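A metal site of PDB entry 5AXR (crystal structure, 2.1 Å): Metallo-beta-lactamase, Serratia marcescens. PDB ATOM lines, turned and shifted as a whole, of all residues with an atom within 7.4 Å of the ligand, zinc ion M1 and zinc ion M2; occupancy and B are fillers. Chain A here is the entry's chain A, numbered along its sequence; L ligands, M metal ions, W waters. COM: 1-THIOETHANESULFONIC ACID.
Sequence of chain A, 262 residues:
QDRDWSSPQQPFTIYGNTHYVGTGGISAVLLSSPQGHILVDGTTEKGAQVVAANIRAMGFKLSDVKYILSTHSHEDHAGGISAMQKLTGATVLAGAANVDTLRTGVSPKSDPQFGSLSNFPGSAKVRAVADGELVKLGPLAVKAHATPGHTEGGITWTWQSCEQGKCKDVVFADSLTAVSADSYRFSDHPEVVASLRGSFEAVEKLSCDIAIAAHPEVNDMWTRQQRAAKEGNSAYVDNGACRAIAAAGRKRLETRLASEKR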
ATOM      1  N   TRP A   5       9.064 -33.058 -33.544  1.00  0.00           N
ATOM      2  CA  TRP A   5       7.883 -32.401 -33.002  1.00  0.00           C
ATOM      3  C   TRP A   5       6.579 -32.926 -33.599  1.00  0.00           C
ATOM      4  O   TRP A   5       5.517 -32.804 -32.978  1.00  0.00           O
ATOM      5  CB  TRP A   5       8.023 -30.888 -33.205  1.00  0.00           C
ATOM      6  CG  TRP A   5       9.167 -30.274 -32.426  1.00  0.00           C
ATOM      7  CD1 TRP A   5       9.849 -30.831 -31.388  1.00  0.00           C
ATOM      8  CD2 TRP A   5       9.735 -28.977 -32.626  1.00  0.00           C
ATOM      9  NE1 TRP A   5      10.798 -29.960 -30.917  1.00  0.00           N
ATOM     10  CE2 TRP A   5      10.739 -28.803 -31.641  1.00  0.00           C
ATOM     11  CE3 TRP A   5       9.463 -27.928 -33.495  1.00  0.00           C
ATOM     12  CZ2 TRP A   5      11.452 -27.613 -31.496  1.00  0.00           C
ATOM     13  CZ3 TRP A   5      10.210 -26.762 -33.385  1.00  0.00           C
ATOM     14  CH2 TRP A   5      11.197 -26.628 -32.403  1.00  0.00           C
ATOM     15  N   GLY A  25       7.697 -35.693 -29.818  1.00  0.00           N
ATOM     16  CA  GLY A  25       8.512 -34.553 -29.334  1.00  0.00           C
ATOM     17  C   GLY A  25       7.809 -33.420 -28.597  1.00  0.00           C
ATOM     18  O   GLY A  25       8.482 -32.568 -28.032  1.00  0.00           O
ATOM     19  N   ILE A  26       6.477 -33.340 -28.729  1.00  0.00           N
ATOM     20  CA  ILE A  26       5.654 -32.288 -28.112  1.00  0.00           C
ATOM     21  C   ILE A  26       4.457 -32.903 -27.352  1.00  0.00           C
ATOM     22  O   ILE A  26       3.709 -33.749 -27.886  1.00  0.00           O
ATOM     23  CB  ILE A  26       5.113 -31.290 -29.161  1.00  0.00           C
ATOM     24  CG1 ILE A  26       6.250 -30.590 -29.932  1.00  0.00           C
ATOM     25  CG2 ILE A  26       4.244 -30.231 -28.504  1.00  0.00           C
ATOM     26  CD1 ILE A  26       7.038 -29.606 -29.084  1.00  0.00           C
ATOM     27  N   HIS A  72       1.408 -21.971 -24.628  1.00  0.00           N
ATOM     28  CA  HIS A  72       1.822 -20.769 -25.323  1.00  0.00           C
ATOM     29  C   HIS A  72       1.784 -20.936 -26.829  1.00  0.00           C
ATOM     30  O   HIS A  72       1.784 -22.060 -27.393  1.00  0.00           O
ATOM     31  CB  HIS A  72       3.223 -20.316 -24.840  1.00  0.00           C
ATOM     32  CG  HIS A  72       4.348 -21.188 -25.296  1.00  0.00           C
ATOM     33  ND1 HIS A  72       4.692 -22.368 -24.668  1.00  0.00           N
ATOM     34  CD2 HIS A  72       5.197 -21.076 -26.348  1.00  0.00           C
ATOM     35  CE1 HIS A  72       5.724 -22.915 -25.282  1.00  0.00           C
ATOM     36  NE2 HIS A  72       6.043 -22.161 -26.311  1.00  0.00           N
ATOM     37  N   SER A  73       1.853 -19.785 -27.487  1.00  0.00           N
ATOM     38  CA  SER A  73       1.506 -19.688 -28.886  1.00  0.00           C
ATOM     39  C   SER A  73       2.727 -19.750 -29.792  1.00  0.00           C
ATOM     40  O   SER A  73       2.930 -18.839 -30.595  1.00  0.00           O
ATOM     41  CB  SER A  73       0.752 -18.365 -29.121  1.00  0.00           C
ATOM     42  OG  SER A  73       1.480 -17.256 -28.622  1.00  0.00           O
ATOM     43  N   HIS A  74       3.585 -20.740 -29.613  1.00  0.00           N
ATOM     44  CA  HIS A  74       4.595 -21.051 -30.607  1.00  0.00           C
ATOM     45  C   HIS A  74       4.088 -22.210 -31.435  1.00  0.00           C
ATOM     46  O   HIS A  74       3.293 -23.021 -30.954  1.00  0.00           O
ATOM     47  CB  HIS A  74       5.921 -21.433 -29.962  1.00  0.00           C
ATOM     48  CG  HIS A  74       6.673 -20.277 -29.409  1.00  0.00           C
ATOM     49  ND1 HIS A  74       7.551 -20.412 -28.361  1.00  0.00           N
ATOM     50  CD2 HIS A  74       6.568 -18.947 -29.644  1.00  0.00           C
ATOM     51  CE1 HIS A  74       8.073 -19.231 -28.082  1.00  0.00           C
ATOM     52  NE2 HIS A  74       7.445 -18.321 -28.798  1.00  0.00           N
ATOM     53  N   GLU A  75       4.659 -22.346 -32.643  1.00  0.00           N
ATOM     54  CA  GLU A  75       4.145 -23.257 -33.662  1.00  0.00           C
ATOM     55  C   GLU A  75       4.232 -24.709 -33.252  1.00  0.00           C
ATOM     56  O   GLU A  75       3.488 -25.550 -33.745  1.00  0.00           O
ATOM     57  CB  GLU A  75       4.911 -23.111 -34.973  1.00  0.00           C
ATOM     58  CG  GLU A  75       4.152 -23.732 -36.150  1.00  0.00           C
ATOM     59  CD  GLU A  75       4.468 -25.205 -36.463  1.00  0.00           C
ATOM     60  OE1 GLU A  75       3.557 -25.916 -36.989  1.00  0.00           O
ATOM     61  OE2 GLU A  75       5.634 -25.645 -36.282  1.00  0.00           O
ATOM     62  N   ASP A  76       5.260 -25.026 -32.465  1.00  0.00           N
ATOM     63  CA  ASP A  76       5.442 -26.402 -32.054  1.00  0.00           C
ATOM     64  C   ASP A  76       4.397 -26.886 -31.037  1.00  0.00           C
ATOM     65  O   ASP A  76       4.199 -28.090 -30.930  1.00  0.00           O
ATOM     66  CB  ASP A  76       6.880 -26.667 -31.624  1.00  0.00           C
ATOM     67  CG  ASP A  76       7.308 -25.843 -30.435  1.00  0.00           C
ATOM     68  OD1 ASP A  76       6.882 -24.685 -30.281  1.00  0.00           O
ATOM     69  OD2 ASP A  76       8.136 -26.366 -29.687  1.00  0.00           O
ATOM     70  N   HIS A  77       3.691 -25.966 -30.367  1.00  0.00           N
ATOM     71  CA  HIS A  77       2.652 -26.331 -29.389  1.00  0.00           C
ATOM     72  C   HIS A  77       1.252 -25.974 -29.872  1.00  0.00           C
ATOM     73  O   HIS A  77       0.272 -26.613 -29.472  1.00  0.00           O
ATOM     74  CB  HIS A  77       2.871 -25.647 -28.043  1.00  0.00           C
ATOM     75  CG  HIS A  77       4.249 -25.823 -27.505  1.00  0.00           C
ATOM     76  ND1 HIS A  77       4.641 -26.972 -26.865  1.00  0.00           N
ATOM     77  CD2 HIS A  77       5.370 -25.077 -27.675  1.00  0.00           C
ATOM     78  CE1 HIS A  77       5.951 -26.937 -26.675  1.00  0.00           C
ATOM     79  NE2 HIS A  77       6.403 -25.770 -27.103  1.00  0.00           N
ATOM     80  N   ASP A 111       7.681 -11.244 -29.071  1.00  0.00           N
ATOM     81  CA  ASP A 111       7.853 -12.658 -28.730  1.00  0.00           C
ATOM     82  C   ASP A 111       9.304 -13.030 -28.951  1.00  0.00           C
ATOM     83  O   ASP A 111       9.835 -12.802 -30.037  1.00  0.00           O
ATOM     84  CB  ASP A 111       6.952 -13.497 -29.634  1.00  0.00           C
ATOM     85  CG  ASP A 111       6.905 -14.966 -29.222  1.00  0.00           C
ATOM     86  OD1 ASP A 111       7.975 -15.611 -29.144  1.00  0.00           O
ATOM     87  OD2 ASP A 111       5.772 -15.475 -29.045  1.00  0.00           O
ATOM     88  N   GLN A 113      10.623 -15.514 -29.968  1.00  0.00           N
ATOM     89  CA  GLN A 113      10.781 -16.289 -31.196  1.00  0.00           C
ATOM     90  C   GLN A 113       9.897 -15.789 -32.322  1.00  0.00           C
ATOM     91  O   GLN A 113       9.597 -16.554 -33.229  1.00  0.00           O
ATOM     92  CB  GLN A 113      10.501 -17.777 -30.925  1.00  0.00           C
ATOM     93  CG  GLN A 113      11.748 -18.632 -31.053  1.00  0.00           C
ATOM     94  CD  GLN A 113      11.951 -19.557 -29.889  1.00  0.00           C
ATOM     95  OE1 GLN A 113      11.413 -19.356 -28.805  1.00  0.00           O
ATOM     96  NE2 GLN A 113      12.751 -20.593 -30.095  1.00  0.00           N
ATOM     97  N   SER A 116      11.903 -16.541 -35.631  1.00  0.00           N
ATOM     98  CA  SER A 116      12.650 -17.794 -35.439  1.00  0.00           C
ATOM     99  C   SER A 116      11.816 -19.035 -35.673  1.00  0.00           C
ATOM    100  O   SER A 116      12.338 -20.085 -36.034  1.00  0.00           O
ATOM    101  CB  SER A 116      13.245 -17.837 -34.016  1.00  0.00           C
ATOM    102  OG  SER A 116      13.476 -19.182 -33.594  1.00  0.00           O
ATOM    103  N   LEU A 117      10.526 -18.947 -35.367  1.00  0.00           N
ATOM    104  CA  LEU A 117       9.558 -19.958 -35.771  1.00  0.00           C
ATOM    105  C   LEU A 117       8.623 -19.329 -36.804  1.00  0.00           C
ATOM    106  O   LEU A 117       8.347 -18.131 -36.756  1.00  0.00           O
ATOM    107  CB  LEU A 117       8.777 -20.475 -34.548  1.00  0.00           C
ATOM    108  CG  LEU A 117       9.599 -21.095 -33.403  1.00  0.00           C
ATOM    109  CD1 LEU A 117       8.736 -21.275 -32.159  1.00  0.00           C
ATOM    110  CD2 LEU A 117      10.215 -22.419 -33.792  1.00  0.00           C
ATOM    111  N   HIS A 150       8.590 -16.776 -21.476  1.00  0.00           N
ATOM    112  CA  HIS A 150       8.995 -17.510 -22.668  1.00  0.00           C
ATOM    113  C   HIS A 150       8.129 -16.998 -23.823  1.00  0.00           C
ATOM    114  O   HIS A 150       8.604 -16.901 -24.945  1.00  0.00           O
ATOM    115  CB  HIS A 150       8.839 -19.009 -22.459  1.00  0.00           C
ATOM    116  CG  HIS A 150       9.058 -19.846 -23.677  1.00  0.00           C
ATOM    117  ND1 HIS A 150      10.269 -20.426 -23.975  1.00  0.00           N
ATOM    118  CD2 HIS A 150       8.183 -20.301 -24.618  1.00  0.00           C
ATOM    119  CE1 HIS A 150      10.145 -21.185 -25.053  1.00  0.00           C
ATOM    120  NE2 HIS A 150       8.894 -21.090 -25.480  1.00  0.00           N
ATOM    121  N   THR A 151       6.884 -16.690 -23.511  1.00  0.00           N
ATOM    122  CA  THR A 151       6.019 -15.763 -24.249  1.00  0.00           C
ATOM    123  C   THR A 151       5.291 -14.958 -23.186  1.00  0.00           C
ATOM    124  O   THR A 151       5.271 -15.354 -22.014  1.00  0.00           O
ATOM    125  CB  THR A 151       4.900 -16.468 -25.079  1.00  0.00           C
ATOM    126  OG1 THR A 151       3.965 -17.115 -24.199  1.00  0.00           O
ATOM    127  CG2 THR A 151       5.458 -17.492 -26.019  1.00  0.00           C
ATOM    128  N   ASP A 174       3.908 -25.098 -18.774  1.00  0.00           N
ATOM    129  CA  ASP A 174       4.401 -24.298 -19.877  1.00  0.00           C
ATOM    130  C   ASP A 174       5.915 -24.162 -19.819  1.00  0.00           C
ATOM    131  O   ASP A 174       6.552 -24.396 -18.775  1.00  0.00           O
ATOM    132  CB  ASP A 174       3.741 -22.929 -19.840  1.00  0.00           C
ATOM    133  CG  ASP A 174       3.989 -22.139 -21.100  1.00  0.00           C
ATOM    134  OD1 ASP A 174       4.285 -22.768 -22.142  1.00  0.00           O
ATOM    135  OD2 ASP A 174       3.953 -20.891 -21.025  1.00  0.00           O
ATOM    136  N   SER A 175       6.502 -23.875 -20.985  1.00  0.00           N
ATOM    137  CA  SER A 175       7.960 -23.733 -21.131  1.00  0.00           C
ATOM    138  C   SER A 175       8.465 -22.510 -20.369  1.00  0.00           C
ATOM    139  O   SER A 175       7.874 -21.437 -20.446  1.00  0.00           O
ATOM    140  CB  SER A 175       8.331 -23.552 -22.614  1.00  0.00           C
ATOM    141  OG  SER A 175       7.891 -24.642 -23.398  1.00  0.00           O
ATOM    142  N   THR A 177      11.806 -21.555 -20.604  1.00  0.00           N
ATOM    143  CA  THR A 177      13.141 -21.525 -21.193  1.00  0.00           C
ATOM    144  C   THR A 177      13.448 -20.174 -21.872  1.00  0.00           C
ATOM    145  O   THR A 177      12.645 -19.647 -22.641  1.00  0.00           O
ATOM    146  CB  THR A 177      13.256 -22.632 -22.250  1.00  0.00           C
ATOM    147  OG1 THR A 177      12.082 -22.608 -23.085  1.00  0.00           O
ATOM    148  CG2 THR A 177      13.378 -23.979 -21.555  1.00  0.00           C
ATOM    149  N   ALA A 178      14.579 -19.585 -21.487  1.00  0.00           N
ATOM    150  CA  ALA A 178      15.106 -18.392 -22.153  1.00  0.00           C
ATOM    151  C   ALA A 178      15.717 -18.775 -23.509  1.00  0.00           C
ATOM    152  O   ALA A 178      16.936 -18.904 -23.610  1.00  0.00           O
ATOM    153  CB  ALA A 178      16.166 -17.743 -21.275  1.00  0.00           C
ATOM    154  N   VAL A 179      14.864 -19.013 -24.500  1.00  0.00           N
ATOM    155  CA  VAL A 179      15.300 -19.310 -25.851  1.00  0.00           C
ATOM    156  C   VAL A 179      14.605 -18.361 -26.812  1.00  0.00           C
ATOM    157  O   VAL A 179      13.532 -17.840 -26.516  1.00  0.00           O
ATOM    158  CB  VAL A 179      14.993 -20.784 -26.263  1.00  0.00           C
ATOM    159  CG1 VAL A 179      15.843 -21.749 -25.463  1.00  0.00           C
ATOM    160  CG2 VAL A 179      13.522 -21.122 -26.103  1.00  0.00           C
ATOM    161  N   SER A 180      15.244 -18.131 -27.954  1.00  0.00           N
ATOM    162  CA  SER A 180      14.785 -17.092 -28.876  1.00  0.00           C
ATOM    163  C   SER A 180      15.381 -17.288 -30.265  1.00  0.00           C
ATOM    164  O   SER A 180      16.332 -18.069 -30.457  1.00  0.00           O
ATOM    165  CB  SER A 180      15.223 -15.730 -28.352  1.00  0.00           C
ATOM    166  OG  SER A 180      16.632 -15.626 -28.324  1.00  0.00           O
ATOM    167  N   ALA A 181      14.914 -16.482 -31.207  1.00  0.00           N
ATOM    168  CA  ALA A 181      15.701 -16.134 -32.394  1.00  0.00           C
ATOM    169  C   ALA A 181      17.131 -15.727 -32.039  1.00  0.00           C
ATOM    170  O   ALA A 181      17.369 -15.135 -30.980  1.00  0.00           O
ATOM    171  CB  ALA A 181      15.022 -15.008 -33.162  1.00  0.00           C
ATOM    172  N   ALA A 214       5.698 -29.209 -21.486  1.00  0.00           N
ATOM    173  CA  ALA A 214       5.282 -28.967 -22.872  1.00  0.00           C
ATOM    174  C   ALA A 214       6.249 -29.636 -23.834  1.00  0.00           C
ATOM    175  O   ALA A 214       5.823 -30.346 -24.745  1.00  0.00           O
ATOM    176  CB  ALA A 214       5.179 -27.475 -23.157  1.00  0.00           C
ATOM    177  N   HIS A 215       7.548 -29.547 -23.522  1.00  0.00           N
ATOM    178  CA  HIS A 215       8.537 -30.477 -24.082  1.00  0.00           C
ATOM    179  C   HIS A 215       8.714 -31.658 -23.145  1.00  0.00           C
ATOM    180  O   HIS A 215       9.356 -31.520 -22.117  1.00  0.00           O
ATOM    181  CB  HIS A 215       9.869 -29.763 -24.360  1.00  0.00           C
ATOM    182  CG  HIS A 215       9.825 -28.852 -25.536  1.00  0.00           C
ATOM    183  ND1 HIS A 215      10.225 -29.257 -26.793  1.00  0.00           N
ATOM    184  CD2 HIS A 215       9.248 -27.626 -25.701  1.00  0.00           C
ATOM    185  CE1 HIS A 215       9.912 -28.324 -27.674  1.00  0.00           C
ATOM    186  NE2 HIS A 215       9.317 -27.326 -27.042  1.00  0.00           N
ATOM    187  N   GLU A 217      10.339 -34.448 -22.609  1.00  0.00           N
ATOM    188  CA  GLU A 217      11.609 -34.899 -22.036  1.00  0.00           C
ATOM    189  C   GLU A 217      12.137 -33.971 -20.937  1.00  0.00           C
ATOM    190  O   GLU A 217      12.973 -34.345 -20.132  1.00  0.00           O
ATOM    191  CB  GLU A 217      12.635 -35.118 -23.159  1.00  0.00           C
ATOM    192  CG  GLU A 217      13.290 -33.877 -23.751  1.00  0.00           C
ATOM    193  CD  GLU A 217      12.392 -32.991 -24.614  1.00  0.00           C
ATOM    194  OE1 GLU A 217      11.321 -33.408 -25.074  1.00  0.00           O
ATOM    195  OE2 GLU A 217      12.785 -31.846 -24.843  1.00  0.00           O
ATOM    196  N   ARG A 252      19.242 -22.059 -16.905  1.00  0.00           N
ATOM    197  CA  ARG A 252      19.317 -21.722 -18.326  1.00  0.00           C
ATOM    198  C   ARG A 252      19.344 -20.207 -18.590  1.00  0.00           C
ATOM    199  O   ARG A 252      20.126 -19.731 -19.389  1.00  0.00           O
ATOM    200  CB  ARG A 252      18.210 -22.382 -19.130  1.00  0.00           C
ATOM    201  CG  ARG A 252      18.274 -22.029 -20.612  1.00  0.00           C
ATOM    202  CD  ARG A 252      17.071 -22.565 -21.348  1.00  0.00           C
ATOM    203  NE  ARG A 252      17.138 -24.014 -21.537  1.00  0.00           N
ATOM    204  CZ  ARG A 252      17.635 -24.600 -22.620  1.00  0.00           C
ATOM    205  NH1 ARG A 252      18.149 -23.885 -23.610  1.00  0.00           N
ATOM    206  NH2 ARG A 252      17.602 -25.920 -22.719  1.00  0.00           N
HETATM  207  C1  COM L   1       9.858 -23.315 -29.220  1.00  0.00           C
HETATM  208  C2  COM L   1      10.758 -24.477 -29.680  1.00  0.00           C
HETATM  209  S1  COM L   1       9.217 -23.527 -27.536  1.00  0.00           S
HETATM  210  S2  COM L   1      12.266 -24.499 -28.963  1.00  0.00           S
HETATM  211  O1S COM L   1      12.766 -22.952 -28.743  1.00  0.00           O
HETATM  212  O2S COM L   1      13.174 -25.189 -29.813  1.00  0.00           O
HETATM  213  O3S COM L   1      12.194 -25.168 -27.682  1.00  0.00           O
HETATM  214 ZN    ZN M   1       7.968 -21.985 -27.119  1.00  0.00          ZN
HETATM  215 ZN    ZN M   2       8.317 -25.644 -27.828  1.00  0.00          ZN
HETATM  216  O   HOH W   1      12.057 -24.633 -24.947  1.00  0.00           O
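The side-chain amide nitrogen (NE2) of Gln 113 sits at hydrogen-bond distance from an oxygen (O1S) of the ligand, 2.7 Å away.
The backbone carbonyl oxygen (O) of Val 179 lies close to the side-chain amide oxygen (OE1) of Gln 113. A ring nitrogen (NE2) of His 74 lies within hydrogen-bond range of the side-chain carboxylate (OD1) of Asp 111, at 2.8 Å. OD1 of Asp 174 is in hydrogen-bond range of ND1 of His 72, 2.6 Å away. The backbone carbonyl oxygen (O) of Thr 177 lies within hydrogen-bond range of a ring nitrogen (ND1) of His 150, 2.8 Å away. The backbone NH of Gln 113 sits at hydrogen-bond distance from the side-chain carboxylate of Asp 111, 2.8 Å away.
Merely in contact with the ligand: Val 179 (3.3 Å), Trp 5 (3.4 Å) and Leu 117 (3.7 Å). Hydrophobic or aromatic side chains that line the ligand: Trp 5, Leu 117, His 150, Val 179 and His 215. Ten residues have an atom within 4 Å of the ligand: Trp 5, His 72, His 74, Asp 76, His 77, Gln 113, Leu 117, His 150, Val 179 and His 215.
Of the 26 residues printed, 3 come within 4 Å of zinc ion M1.
Of the 26 residues printed, 3 come within 4 Å of zinc ion M2.
S1 of the ligand binds zinc ion M1 (2.0 Å). Zinc ion M1 is bound by a ring nitrogen (ND1) of His 74, 2.0 Å away. Zinc ion M1 is bound by a ring nitrogen (NE2) of His 150 (2.1 Å). NE2 of His 72 is bound to zinc ion M1 (2.1 Å). Zinc ion M1 has four donor atoms within binding distance.
OD2 of Asp 76 is bound to zinc ion M2, 2.0 Å away. A ring nitrogen (NE2) of His 77 is bound to zinc ion M2 (2.1 Å). NE2 of His 215 is bound to zinc ion M2 (2.1 Å). S1 of the ligand is bound to zinc ion M2 (2.3 Å). Zinc ion M2 has four donor atoms within binding distance.
Water W1 bridges the side-chain hydroxyl of Thr 177 and an oxygen (O3S) of the ligand.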
